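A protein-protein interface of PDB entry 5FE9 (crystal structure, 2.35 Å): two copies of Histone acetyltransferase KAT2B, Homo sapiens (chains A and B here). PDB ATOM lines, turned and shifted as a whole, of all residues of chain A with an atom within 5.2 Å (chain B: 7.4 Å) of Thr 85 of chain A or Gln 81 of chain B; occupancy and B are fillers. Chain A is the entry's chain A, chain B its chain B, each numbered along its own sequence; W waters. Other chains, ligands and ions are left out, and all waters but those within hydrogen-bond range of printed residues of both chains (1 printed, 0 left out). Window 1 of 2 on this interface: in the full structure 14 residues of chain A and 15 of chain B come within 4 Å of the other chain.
Thr 85 of chain A touches just one residue of chain B: Gln 81 (3.2 Å).
Asn 86 of chain A touches none of the printed residues of chain B.
Of the printed residues of chain A, Met 77 of chain B touches Glu 89.
Gln 81 of chain B touches one residue of chain A.
Of the printed residues of chain A, Phe 109 of chain B touches Lys 88 and Glu 89.
The nearest residue of chain B that does not touch Thr 85 of chain A is Phe 109 of chain B (4.1 Å).
The nearest residue of chain A that does not touch Gln 81 of chain B is Gln 81 of chain A (4.6 Å).
The nearest printed residue of chain A that does not touch Lys 88 of chain B is Gln 81 of chain A (5.5 Å).
Thr 85 of chain A touches Gln 81 of chain B, but with the chains exchanged Gln 81 of chain A does not touch Thr 85 of chain B (4.02 Å).
Lys 88 of chain B touches its own counterpart, Lys 88 of chain A.
Positions printed for both chains: 81, 82, 83, 84, 85, 86, 87 and 88.
Of the 6 pairs that touch across the chains among the printed residues, 1 has its exchanged pair printed and touching as well.
Among the printed residues, pairs that only touch across the chains: Thr 85 of chain A with Gln 81 of chain B (3.2 Å), Lys 88 of chain A with Phe 109 of chain B (3.5 Å), Glu 89 of chain A with Met 77 of chain B (3.4 Å) and Glu 89 of chain A with Phe 109 of chain B (3.6 Å).
The side-chain carboxylate (OE2) of Glu 105 of chain B lies close to the side-chain amide oxygen (OE1) of Gln 81 of chain B, 3.3 Å away.
The side-chain amino group of Lys 88 of chain B lies within salt-bridge range of the side-chain carboxylate of Glu 105 of chain B (3.4 Å).
Printed residues of chain A that touch a printed residue of chain B: Thr 85, Lys 88 and Glu 89.
Along chain A the printed residues that touch a printed residue of chain B span positions 85 to 89.
Printed residues of chain B that touch a printed residue of chain A: Met 77, Gln 81, Lys 88, Glu 105 and Phe 109.
Hydrophobic or aromatic side chains of chain B that line the printed part of chain A: Met 77 and Phe 109.
Along chain B the printed residues that touch a printed residue of chain A span positions 77 to 109.
Among the printed residues, 6 pairs touch across the chains.
Among the printed residues, Asp or Glu carboxylates within 4 Å of a Lys or Arg side-chain nitrogen of the other chain: Lys 88 of chain A with Glu 105 of chain B (2.8 Å).
The side-chain amino group (NZ) of Lys 88 of chain A lies close to the side-chain amino group (NZ) of Lys 88 of chain B, at 3.3 Å.
The side-chain amino group of Lys 88 of chain A is in salt-bridge range of the side-chain carboxylate of Glu 105 of chain B, 2.8 Å away.
Water W1 lies within hydrogen-bond range of the backbone carbonyl oxygen of Phe 109 of chain B (2.9 Å) and the backbone carbonyl oxygen of Glu 89 of chain A (2.9 Å).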
ATOM      1  N   GLN A  81      17.759 -20.085 -10.921  1.00  0.00           N
ATOM      2  CA  GLN A  81      17.161 -20.103  -9.605  1.00  0.00           C
ATOM      3  C   GLN A  81      16.521 -21.459  -9.272  1.00  0.00           C
ATOM      4  O   GLN A  81      16.653 -21.967  -8.154  1.00  0.00           O
ATOM      5  CB  GLN A  81      16.150 -18.944  -9.476  1.00  0.00           C
ATOM      6  CG  GLN A  81      15.652 -18.728  -8.071  1.00  0.00           C
ATOM      7  CD  GLN A  81      16.751 -18.292  -7.138  1.00  0.00           C
ATOM      8  OE1 GLN A  81      17.194 -17.143  -7.195  1.00  0.00           O
ATOM      9  NE2 GLN A  81      17.161 -19.183  -6.221  1.00  0.00           N
ATOM     10  N   ARG A  82      15.857 -22.047 -10.247  1.00  0.00           N
ATOM     11  CA  ARG A  82      15.258 -23.349 -10.099  1.00  0.00           C
ATOM     12  C   ARG A  82      16.244 -24.468  -9.789  1.00  0.00           C
ATOM     13  O   ARG A  82      15.923 -25.401  -9.082  1.00  0.00           O
ATOM     14  CB  ARG A  82      14.525 -23.705 -11.367  1.00  0.00           C
ATOM     15  CG  ARG A  82      13.580 -24.874 -11.111  1.00  0.00           C
ATOM     16  CD  ARG A  82      12.254 -24.697 -11.805  1.00  0.00           C
ATOM     17  NE  ARG A  82      12.549 -24.688 -13.239  1.00  0.00           N
ATOM     18  CZ  ARG A  82      12.539 -23.615 -14.048  1.00  0.00           C
ATOM     19  NH1 ARG A  82      12.908 -23.783 -15.324  1.00  0.00           N
ATOM     20  NH2 ARG A  82      12.123 -22.394 -13.634  1.00  0.00           N
ATOM     21  N   VAL A  83      17.440 -24.379 -10.334  1.00  0.00           N
ATOM     22  CA  VAL A  83      18.477 -25.336  -9.988  1.00  0.00           C
ATOM     23  C   VAL A  83      18.659 -25.362  -8.470  1.00  0.00           C
ATOM     24  O   VAL A  83      18.772 -26.434  -7.847  1.00  0.00           O
ATOM     25  CB  VAL A  83      19.825 -24.977 -10.654  1.00  0.00           C
ATOM     26  CG1 VAL A  83      20.952 -25.871 -10.118  1.00  0.00           C
ATOM     27  CG2 VAL A  83      19.740 -25.086 -12.171  1.00  0.00           C
ATOM     28  N   PHE A  84      18.686 -24.168  -7.879  1.00  0.00           N
ATOM     29  CA  PHE A  84      18.941 -24.046  -6.449  1.00  0.00           C
ATOM     30  C   PHE A  84      17.753 -24.452  -5.632  1.00  0.00           C
ATOM     31  O   PHE A  84      17.903 -25.156  -4.665  1.00  0.00           O
ATOM     32  CB  PHE A  84      19.373 -22.630  -6.094  1.00  0.00           C
ATOM     33  CG  PHE A  84      20.530 -22.144  -6.884  1.00  0.00           C
ATOM     34  CD1 PHE A  84      21.617 -22.945  -7.049  1.00  0.00           C
ATOM     35  CD2 PHE A  84      20.535 -20.856  -7.430  1.00  0.00           C
ATOM     36  CE1 PHE A  84      22.666 -22.522  -7.784  1.00  0.00           C
ATOM     37  CE2 PHE A  84      21.598 -20.420  -8.160  1.00  0.00           C
ATOM     38  CZ  PHE A  84      22.663 -21.250  -8.342  1.00  0.00           C
ATOM     39  N   THR A  85      16.567 -24.021  -6.033  1.00  0.00           N
ATOM     40  CA  THR A  85      15.387 -24.257  -5.218  1.00  0.00           C
ATOM     41  C   THR A  85      14.974 -25.735  -5.267  1.00  0.00           C
ATOM     42  O   THR A  85      14.466 -26.280  -4.276  1.00  0.00           O
ATOM     43  CB  THR A  85      14.219 -23.305  -5.598  1.00  0.00           C
ATOM     44  OG1 THR A  85      13.768 -23.559  -6.933  1.00  0.00           O
ATOM     45  CG2 THR A  85      14.653 -21.833  -5.479  1.00  0.00           C
ATOM     46  N   ASN A  86      15.193 -26.385  -6.414  1.00  0.00           N
ATOM     47  CA  ASN A  86      15.003 -27.839  -6.516  1.00  0.00           C
ATOM     48  C   ASN A  86      15.903 -28.576  -5.510  1.00  0.00           C
ATOM     49  O   ASN A  86      15.455 -29.408  -4.710  1.00  0.00           O
ATOM     50  CB  ASN A  86      15.336 -28.342  -7.919  1.00  0.00           C
ATOM     51  CG  ASN A  86      14.300 -27.965  -8.970  1.00  0.00           C
ATOM     52  OD1 ASN A  86      13.194 -27.528  -8.667  1.00  0.00           O
ATOM     53  ND2 ASN A  86      14.673 -28.150 -10.231  1.00  0.00           N
ATOM     54  N   CYS A  87      17.169 -28.234  -5.543  1.00  0.00           N
ATOM     55  CA  CYS A  87      18.138 -28.837  -4.653  1.00  0.00           C
ATOM     56  C   CYS A  87      17.766 -28.638  -3.181  1.00  0.00           C
ATOM     57  O   CYS A  87      17.857 -29.577  -2.380  1.00  0.00           O
ATOM     58  CB  CYS A  87      19.512 -28.235  -4.932  1.00  0.00           C
ATOM     59  SG  CYS A  87      20.804 -28.920  -3.891  1.00  0.00           S
ATOM     60  N   LYS A  88      17.337 -27.428  -2.828  1.00  0.00           N
ATOM     61  CA  LYS A  88      17.039 -27.130  -1.449  1.00  0.00           C
ATOM     62  C   LYS A  88      15.773 -27.791  -0.972  1.00  0.00           C
ATOM     63  O   LYS A  88      15.698 -28.151   0.223  1.00  0.00           O
ATOM     64  CB  LYS A  88      17.007 -25.634  -1.212  1.00  0.00           C
ATOM     65  CG  LYS A  88      18.383 -25.054  -1.326  1.00  0.00           C
ATOM     66  CD  LYS A  88      18.487 -23.606  -0.821  1.00  0.00           C
ATOM     67  CE  LYS A  88      18.644 -22.649  -1.961  1.00  0.00           C
ATOM     68  NZ  LYS A  88      18.688 -21.246  -1.511  1.00  0.00           N
ATOM     69  N   GLU A  89      14.785 -27.943  -1.873  1.00  0.00           N
ATOM     70  CA  GLU A  89      13.535 -28.661  -1.506  1.00  0.00           C
ATOM     71  C   GLU A  89      13.804 -30.142  -1.263  1.00  0.00           C
ATOM     72  O   GLU A  89      13.297 -30.710  -0.292  1.00  0.00           O
ATOM     73  CB  GLU A  89      12.371 -28.462  -2.529  1.00  0.00           C
ATOM     74  CG  GLU A  89      11.329 -29.594  -2.656  1.00  0.00           C
ATOM     75  CD  GLU A  89       9.934 -29.046  -3.003  1.00  0.00           C
ATOM     76  OE1 GLU A  89       9.882 -28.220  -3.944  1.00  0.00           O
ATOM     77  OE2 GLU A  89       8.907 -29.421  -2.343  1.00  0.00           O
ATOM     78  N   TYR A  90      14.593 -30.754  -2.153  1.00  0.00           N
ATOM     79  CA  TYR A  90      14.813 -32.192  -2.128  1.00  0.00           C
ATOM     80  C   TYR A  90      15.767 -32.640  -1.030  1.00  0.00           C
ATOM     81  O   TYR A  90      15.523 -33.625  -0.376  1.00  0.00           O
ATOM     82  CB  TYR A  90      15.330 -32.666  -3.465  1.00  0.00           C
ATOM     83  CG  TYR A  90      15.369 -34.165  -3.551  1.00  0.00           C
ATOM     84  CD1 TYR A  90      14.179 -34.898  -3.663  1.00  0.00           C
ATOM     85  CD2 TYR A  90      16.590 -34.875  -3.476  1.00  0.00           C
ATOM     86  CE1 TYR A  90      14.201 -36.289  -3.695  1.00  0.00           C
ATOM     87  CE2 TYR A  90      16.617 -36.261  -3.513  1.00  0.00           C
ATOM     88  CZ  TYR A  90      15.422 -36.964  -3.628  1.00  0.00           C
ATOM     89  OH  TYR A  90      15.451 -38.334  -3.716  1.00  0.00           O
ATOM     90  N   MET B  56       6.566  -9.420  -1.741  1.00  0.00           N
ATOM     91  CA  MET B  56       5.798 -10.410  -1.007  1.00  0.00           C
ATOM     92  C   MET B  56       6.265 -10.432   0.448  1.00  0.00           C
ATOM     93  O   MET B  56       7.394 -10.077   0.773  1.00  0.00           O
ATOM     94  CB  MET B  56       5.907 -11.794  -1.668  1.00  0.00           C
ATOM     95  CG  MET B  56       4.961 -12.873  -1.114  1.00  0.00           C
ATOM     96  SD  MET B  56       3.237 -12.377  -0.849  1.00  0.00           S
ATOM     97  CE  MET B  56       2.792 -11.856  -2.498  1.00  0.00           C
ATOM     98  N   MET B  61       0.760 -13.108   2.705  1.00  0.00           N
ATOM     99  CA  MET B  61       0.524 -14.526   2.586  1.00  0.00           C
ATOM    100  C   MET B  61      -0.581 -15.032   3.522  1.00  0.00           C
ATOM    101  O   MET B  61      -1.384 -15.908   3.121  1.00  0.00           O
ATOM    102  CB  MET B  61       1.805 -15.314   2.816  1.00  0.00           C
ATOM    103  CG  MET B  61       2.762 -15.267   1.628  1.00  0.00           C
ATOM    104  SD  MET B  61       4.080 -16.502   1.699  1.00  0.00           S
ATOM    105  CE  MET B  61       3.172 -18.016   1.351  1.00  0.00           C
ATOM    106  N   LEU B  75       1.351 -22.727  -5.691  1.00  0.00           N
ATOM    107  CA  LEU B  75       1.080 -21.288  -5.478  1.00  0.00           C
ATOM    108  C   LEU B  75       1.638 -20.775  -4.163  1.00  0.00           C
ATOM    109  O   LEU B  75       2.163 -19.657  -4.101  1.00  0.00           O
ATOM    110  CB  LEU B  75      -0.415 -20.979  -5.533  1.00  0.00           C
ATOM    111  CG  LEU B  75      -1.059 -21.084  -6.909  1.00  0.00           C
ATOM    112  CD1 LEU B  75      -2.580 -21.112  -6.777  1.00  0.00           C
ATOM    113  CD2 LEU B  75      -0.598 -19.945  -7.823  1.00  0.00           C
ATOM    114  N   PHE B  76       1.496 -21.591  -3.120  1.00  0.00           N
ATOM    115  CA  PHE B  76       2.032 -21.281  -1.801  1.00  0.00           C
ATOM    116  C   PHE B  76       3.554 -21.212  -1.846  1.00  0.00           C
ATOM    117  O   PHE B  76       4.139 -20.274  -1.346  1.00  0.00           O
ATOM    118  CB  PHE B  76       1.537 -22.334  -0.773  1.00  0.00           C
ATOM    119  CG  PHE B  76       1.964 -22.060   0.648  1.00  0.00           C
ATOM    120  CD1 PHE B  76       1.244 -21.191   1.444  1.00  0.00           C
ATOM    121  CD2 PHE B  76       3.044 -22.733   1.205  1.00  0.00           C
ATOM    122  CE1 PHE B  76       1.628 -20.949   2.754  1.00  0.00           C
ATOM    123  CE2 PHE B  76       3.427 -22.510   2.515  1.00  0.00           C
ATOM    124  CZ  PHE B  76       2.728 -21.603   3.288  1.00  0.00           C
ATOM    125  N   MET B  77       4.168 -22.213  -2.461  1.00  0.00           N
ATOM    126  CA  MET B  77       5.628 -22.298  -2.605  1.00  0.00           C
ATOM    127  C   MET B  77       6.177 -21.075  -3.345  1.00  0.00           C
ATOM    128  O   MET B  77       7.195 -20.533  -2.971  1.00  0.00           O
ATOM    129  CB  MET B  77       6.045 -23.548  -3.409  1.00  0.00           C
ATOM    130  CG  MET B  77       5.638 -24.887  -2.816  1.00  0.00           C
ATOM    131  SD  MET B  77       6.590 -25.314  -1.378  1.00  0.00           S
ATOM    132  CE  MET B  77       8.111 -25.900  -2.125  1.00  0.00           C
ATOM    133  N   ALA B  78       5.498 -20.649  -4.393  1.00  0.00           N
ATOM    134  CA  ALA B  78       6.015 -19.553  -5.197  1.00  0.00           C
ATOM    135  C   ALA B  78       6.025 -18.233  -4.409  1.00  0.00           C
ATOM    136  O   ALA B  78       6.964 -17.438  -4.541  1.00  0.00           O
ATOM    137  CB  ALA B  78       5.232 -19.405  -6.503  1.00  0.00           C
ATOM    138  N   ASP B  79       4.984 -18.011  -3.604  1.00  0.00           N
ATOM    139  CA  ASP B  79       4.863 -16.779  -2.837  1.00  0.00           C
ATOM    140  C   ASP B  79       5.924 -16.755  -1.769  1.00  0.00           C
ATOM    141  O   ASP B  79       6.616 -15.754  -1.600  1.00  0.00           O
ATOM    142  CB  ASP B  79       3.487 -16.652  -2.199  1.00  0.00           C
ATOM    143  CG  ASP B  79       2.455 -16.091  -3.145  1.00  0.00           C
ATOM    144  OD1 ASP B  79       2.790 -15.817  -4.338  1.00  0.00           O
ATOM    145  OD2 ASP B  79       1.297 -15.905  -2.701  1.00  0.00           O
ATOM    146  N   LEU B  80       6.083 -17.870  -1.058  1.00  0.00           N
ATOM    147  CA  LEU B  80       7.072 -17.910  -0.015  1.00  0.00           C
ATOM    148  C   LEU B  80       8.471 -17.816  -0.599  1.00  0.00           C
ATOM    149  O   LEU B  80       9.333 -17.160  -0.047  1.00  0.00           O
ATOM    150  CB  LEU B  80       6.875 -19.144   0.866  1.00  0.00           C
ATOM    151  CG  LEU B  80       7.587 -19.280   2.231  1.00  0.00           C
ATOM    152  CD1 LEU B  80       7.937 -17.966   2.871  1.00  0.00           C
ATOM    153  CD2 LEU B  80       6.705 -20.093   3.191  1.00  0.00           C
ATOM    154  N   GLN B  81       8.701 -18.482  -1.710  1.00  0.00           N
ATOM    155  CA  GLN B  81      10.008 -18.430  -2.381  1.00  0.00           C
ATOM    156  C   GLN B  81      10.363 -16.995  -2.858  1.00  0.00           C
ATOM    157  O   GLN B  81      11.472 -16.571  -2.712  1.00  0.00           O
ATOM    158  CB  GLN B  81      10.044 -19.437  -3.537  1.00  0.00           C
ATOM    159  CG  GLN B  81      11.426 -19.636  -4.175  1.00  0.00           C
ATOM    160  CD  GLN B  81      12.550 -20.099  -3.186  1.00  0.00           C
ATOM    161  OE1 GLN B  81      13.685 -19.639  -3.320  1.00  0.00           O
ATOM    162  NE2 GLN B  81      12.221 -20.947  -2.163  1.00  0.00           N
ATOM    163  N   ARG B  82       9.383 -16.256  -3.331  1.00  0.00           N
ATOM    164  CA  ARG B  82       9.528 -14.850  -3.719  1.00  0.00           C
ATOM    165  C   ARG B  82       9.946 -13.943  -2.563  1.00  0.00           C
ATOM    166  O   ARG B  82      10.676 -12.993  -2.759  1.00  0.00           O
ATOM    167  CB  ARG B  82       8.173 -14.369  -4.270  1.00  0.00           C
ATOM    168  CG  ARG B  82       7.970 -12.922  -4.696  1.00  0.00           C
ATOM    169  CD  ARG B  82       8.703 -12.502  -5.966  1.00  0.00           C
ATOM    170  NE  ARG B  82       8.440 -13.279  -7.176  1.00  0.00           N
ATOM    171  CZ  ARG B  82       9.107 -13.121  -8.332  1.00  0.00           C
ATOM    172  NH1 ARG B  82      10.110 -12.244  -8.438  1.00  0.00           N
ATOM    173  NH2 ARG B  82       8.783 -13.863  -9.388  1.00  0.00           N
ATOM    174  N   VAL B  83       9.451 -14.225  -1.351  1.00  0.00           N
ATOM    175  CA  VAL B  83       9.913 -13.530  -0.183  1.00  0.00           C
ATOM    176  C   VAL B  83      11.442 -13.629  -0.104  1.00  0.00           C
ATOM    177  O   VAL B  83      12.143 -12.637   0.172  1.00  0.00           O
ATOM    178  CB  VAL B  83       9.301 -14.106   1.114  1.00  0.00           C
ATOM    179  CG1 VAL B  83       9.938 -13.458   2.355  1.00  0.00           C
ATOM    180  CG2 VAL B  83       7.788 -13.917   1.136  1.00  0.00           C
ATOM    181  N   PHE B  84      11.957 -14.838  -0.344  1.00  0.00           N
ATOM    182  CA  PHE B  84      13.398 -15.120  -0.190  1.00  0.00           C
ATOM    183  C   PHE B  84      14.190 -14.551  -1.348  1.00  0.00           C
ATOM    184  O   PHE B  84      15.189 -13.909  -1.138  1.00  0.00           O
ATOM    185  CB  PHE B  84      13.678 -16.625  -0.001  1.00  0.00           C
ATOM    186  CG  PHE B  84      12.923 -17.262   1.167  1.00  0.00           C
ATOM    187  CD1 PHE B  84      12.830 -16.614   2.397  1.00  0.00           C
ATOM    188  CD2 PHE B  84      12.322 -18.520   1.056  1.00  0.00           C
ATOM    189  CE1 PHE B  84      12.148 -17.183   3.466  1.00  0.00           C
ATOM    190  CE2 PHE B  84      11.636 -19.091   2.129  1.00  0.00           C
ATOM    191  CZ  PHE B  84      11.538 -18.428   3.320  1.00  0.00           C
ATOM    192  N   THR B  85      13.694 -14.705  -2.561  1.00  0.00           N
ATOM    193  CA  THR B  85      14.425 -14.235  -3.744  1.00  0.00           C
ATOM    194  C   THR B  85      14.422 -12.675  -3.866  1.00  0.00           C
ATOM    195  O   THR B  85      15.405 -12.085  -4.306  1.00  0.00           O
ATOM    196  CB  THR B  85      13.916 -14.911  -5.041  1.00  0.00           C
ATOM    197  OG1 THR B  85      12.584 -14.497  -5.331  1.00  0.00           O
ATOM    198  CG2 THR B  85      13.960 -16.449  -4.914  1.00  0.00           C
ATOM    199  N   ASN B  86      13.347 -12.016  -3.453  1.00  0.00           N
ATOM    200  CA  ASN B  86      13.345 -10.540  -3.332  1.00  0.00           C
ATOM    201  C   ASN B  86      14.456 -10.081  -2.391  1.00  0.00           C
ATOM    202  O   ASN B  86      15.235  -9.187  -2.717  1.00  0.00           O
ATOM    203  CB  ASN B  86      11.997 -10.026  -2.786  1.00  0.00           C
ATOM    204  CG  ASN B  86      10.892 -10.094  -3.807  1.00  0.00           C
ATOM    205  OD1 ASN B  86      11.143 -10.293  -5.010  1.00  0.00           O
ATOM    206  ND2 ASN B  86       9.665  -9.934  -3.349  1.00  0.00           N
ATOM    207  N   CYS B  87      14.491 -10.697  -1.223  1.00  0.00           N
ATOM    208  CA  CYS B  87      15.462 -10.371  -0.217  1.00  0.00           C
ATOM    209  C   CYS B  87      16.887 -10.566  -0.730  1.00  0.00           C
ATOM    210  O   CYS B  87      17.743  -9.706  -0.520  1.00  0.00           O
ATOM    211  CB  CYS B  87      15.214 -11.212   1.031  1.00  0.00           C
ATOM    212  SG  CYS B  87      16.373 -10.868   2.357  1.00  0.00           S
ATOM    213  N   LYS B  88      17.137 -11.662  -1.448  1.00  0.00           N
ATOM    214  CA  LYS B  88      18.476 -11.942  -1.943  1.00  0.00           C
ATOM    215  C   LYS B  88      18.874 -11.073  -3.131  1.00  0.00           C
ATOM    216  O   LYS B  88      20.042 -10.747  -3.289  1.00  0.00           O
ATOM    217  CB  LYS B  88      18.596 -13.408  -2.273  1.00  0.00           C
ATOM    218  CG  LYS B  88      18.470 -14.300  -1.043  1.00  0.00           C
ATOM    219  CD  LYS B  88      18.590 -15.708  -1.498  1.00  0.00           C
ATOM    220  CE  LYS B  88      18.113 -16.644  -0.455  1.00  0.00           C
ATOM    221  NZ  LYS B  88      18.161 -18.044  -0.921  1.00  0.00           N
ATOM    222  N   GLU B 105      14.451 -20.165   5.030  1.00  0.00           N
ATOM    223  CA  GLU B 105      14.244 -21.061   3.900  1.00  0.00           C
ATOM    224  C   GLU B 105      14.527 -22.507   4.267  1.00  0.00           C
ATOM    225  O   GLU B 105      13.786 -23.399   3.875  1.00  0.00           O
ATOM    226  CB  GLU B 105      15.109 -20.640   2.733  1.00  0.00           C
ATOM    227  CG  GLU B 105      14.859 -21.438   1.468  1.00  0.00           C
ATOM    228  CD  GLU B 105      15.809 -21.054   0.376  1.00  0.00           C
ATOM    229  OE1 GLU B 105      16.984 -20.850   0.678  1.00  0.00           O
ATOM    230  OE2 GLU B 105      15.392 -21.004  -0.815  1.00  0.00           O
ATOM    231  N   PHE B 108      11.587 -23.570   6.470  1.00  0.00           N
ATOM    232  CA  PHE B 108      10.518 -23.766   5.499  1.00  0.00           C
ATOM    233  C   PHE B 108      10.574 -25.122   4.814  1.00  0.00           C
ATOM    234  O   PHE B 108       9.609 -25.888   4.864  1.00  0.00           O
ATOM    235  CB  PHE B 108      10.567 -22.622   4.499  1.00  0.00           C
ATOM    236  CG  PHE B 108       9.837 -22.877   3.222  1.00  0.00           C
ATOM    237  CD1 PHE B 108       8.451 -23.025   3.198  1.00  0.00           C
ATOM    238  CD2 PHE B 108      10.530 -22.858   1.995  1.00  0.00           C
ATOM    239  CE1 PHE B 108       7.777 -23.167   1.989  1.00  0.00           C
ATOM    240  CE2 PHE B 108       9.856 -22.992   0.792  1.00  0.00           C
ATOM    241  CZ  PHE B 108       8.479 -23.166   0.792  1.00  0.00           C
ATOM    242  N   PHE B 109      11.703 -25.449   4.193  1.00  0.00           N
ATOM    243  CA  PHE B 109      11.775 -26.707   3.464  1.00  0.00           C
ATOM    244  C   PHE B 109      11.654 -27.915   4.388  1.00  0.00           C
ATOM    245  O   PHE B 109      11.132 -28.941   3.977  1.00  0.00           O
ATOM    246  CB  PHE B 109      13.036 -26.784   2.600  1.00  0.00           C
ATOM    247  CG  PHE B 109      12.970 -25.929   1.359  1.00  0.00           C
ATOM    248  CD1 PHE B 109      11.953 -26.090   0.450  1.00  0.00           C
ATOM    249  CD2 PHE B 109      13.976 -25.004   1.072  1.00  0.00           C
ATOM    250  CE1 PHE B 109      11.909 -25.326  -0.708  1.00  0.00           C
ATOM    251  CE2 PHE B 109      13.945 -24.247  -0.091  1.00  0.00           C
ATOM    252  CZ  PHE B 109      12.902 -24.395  -0.973  1.00  0.00           C
HETATM  253  O   HOH W   1      10.993 -30.043   1.328  1.00  0.00           O
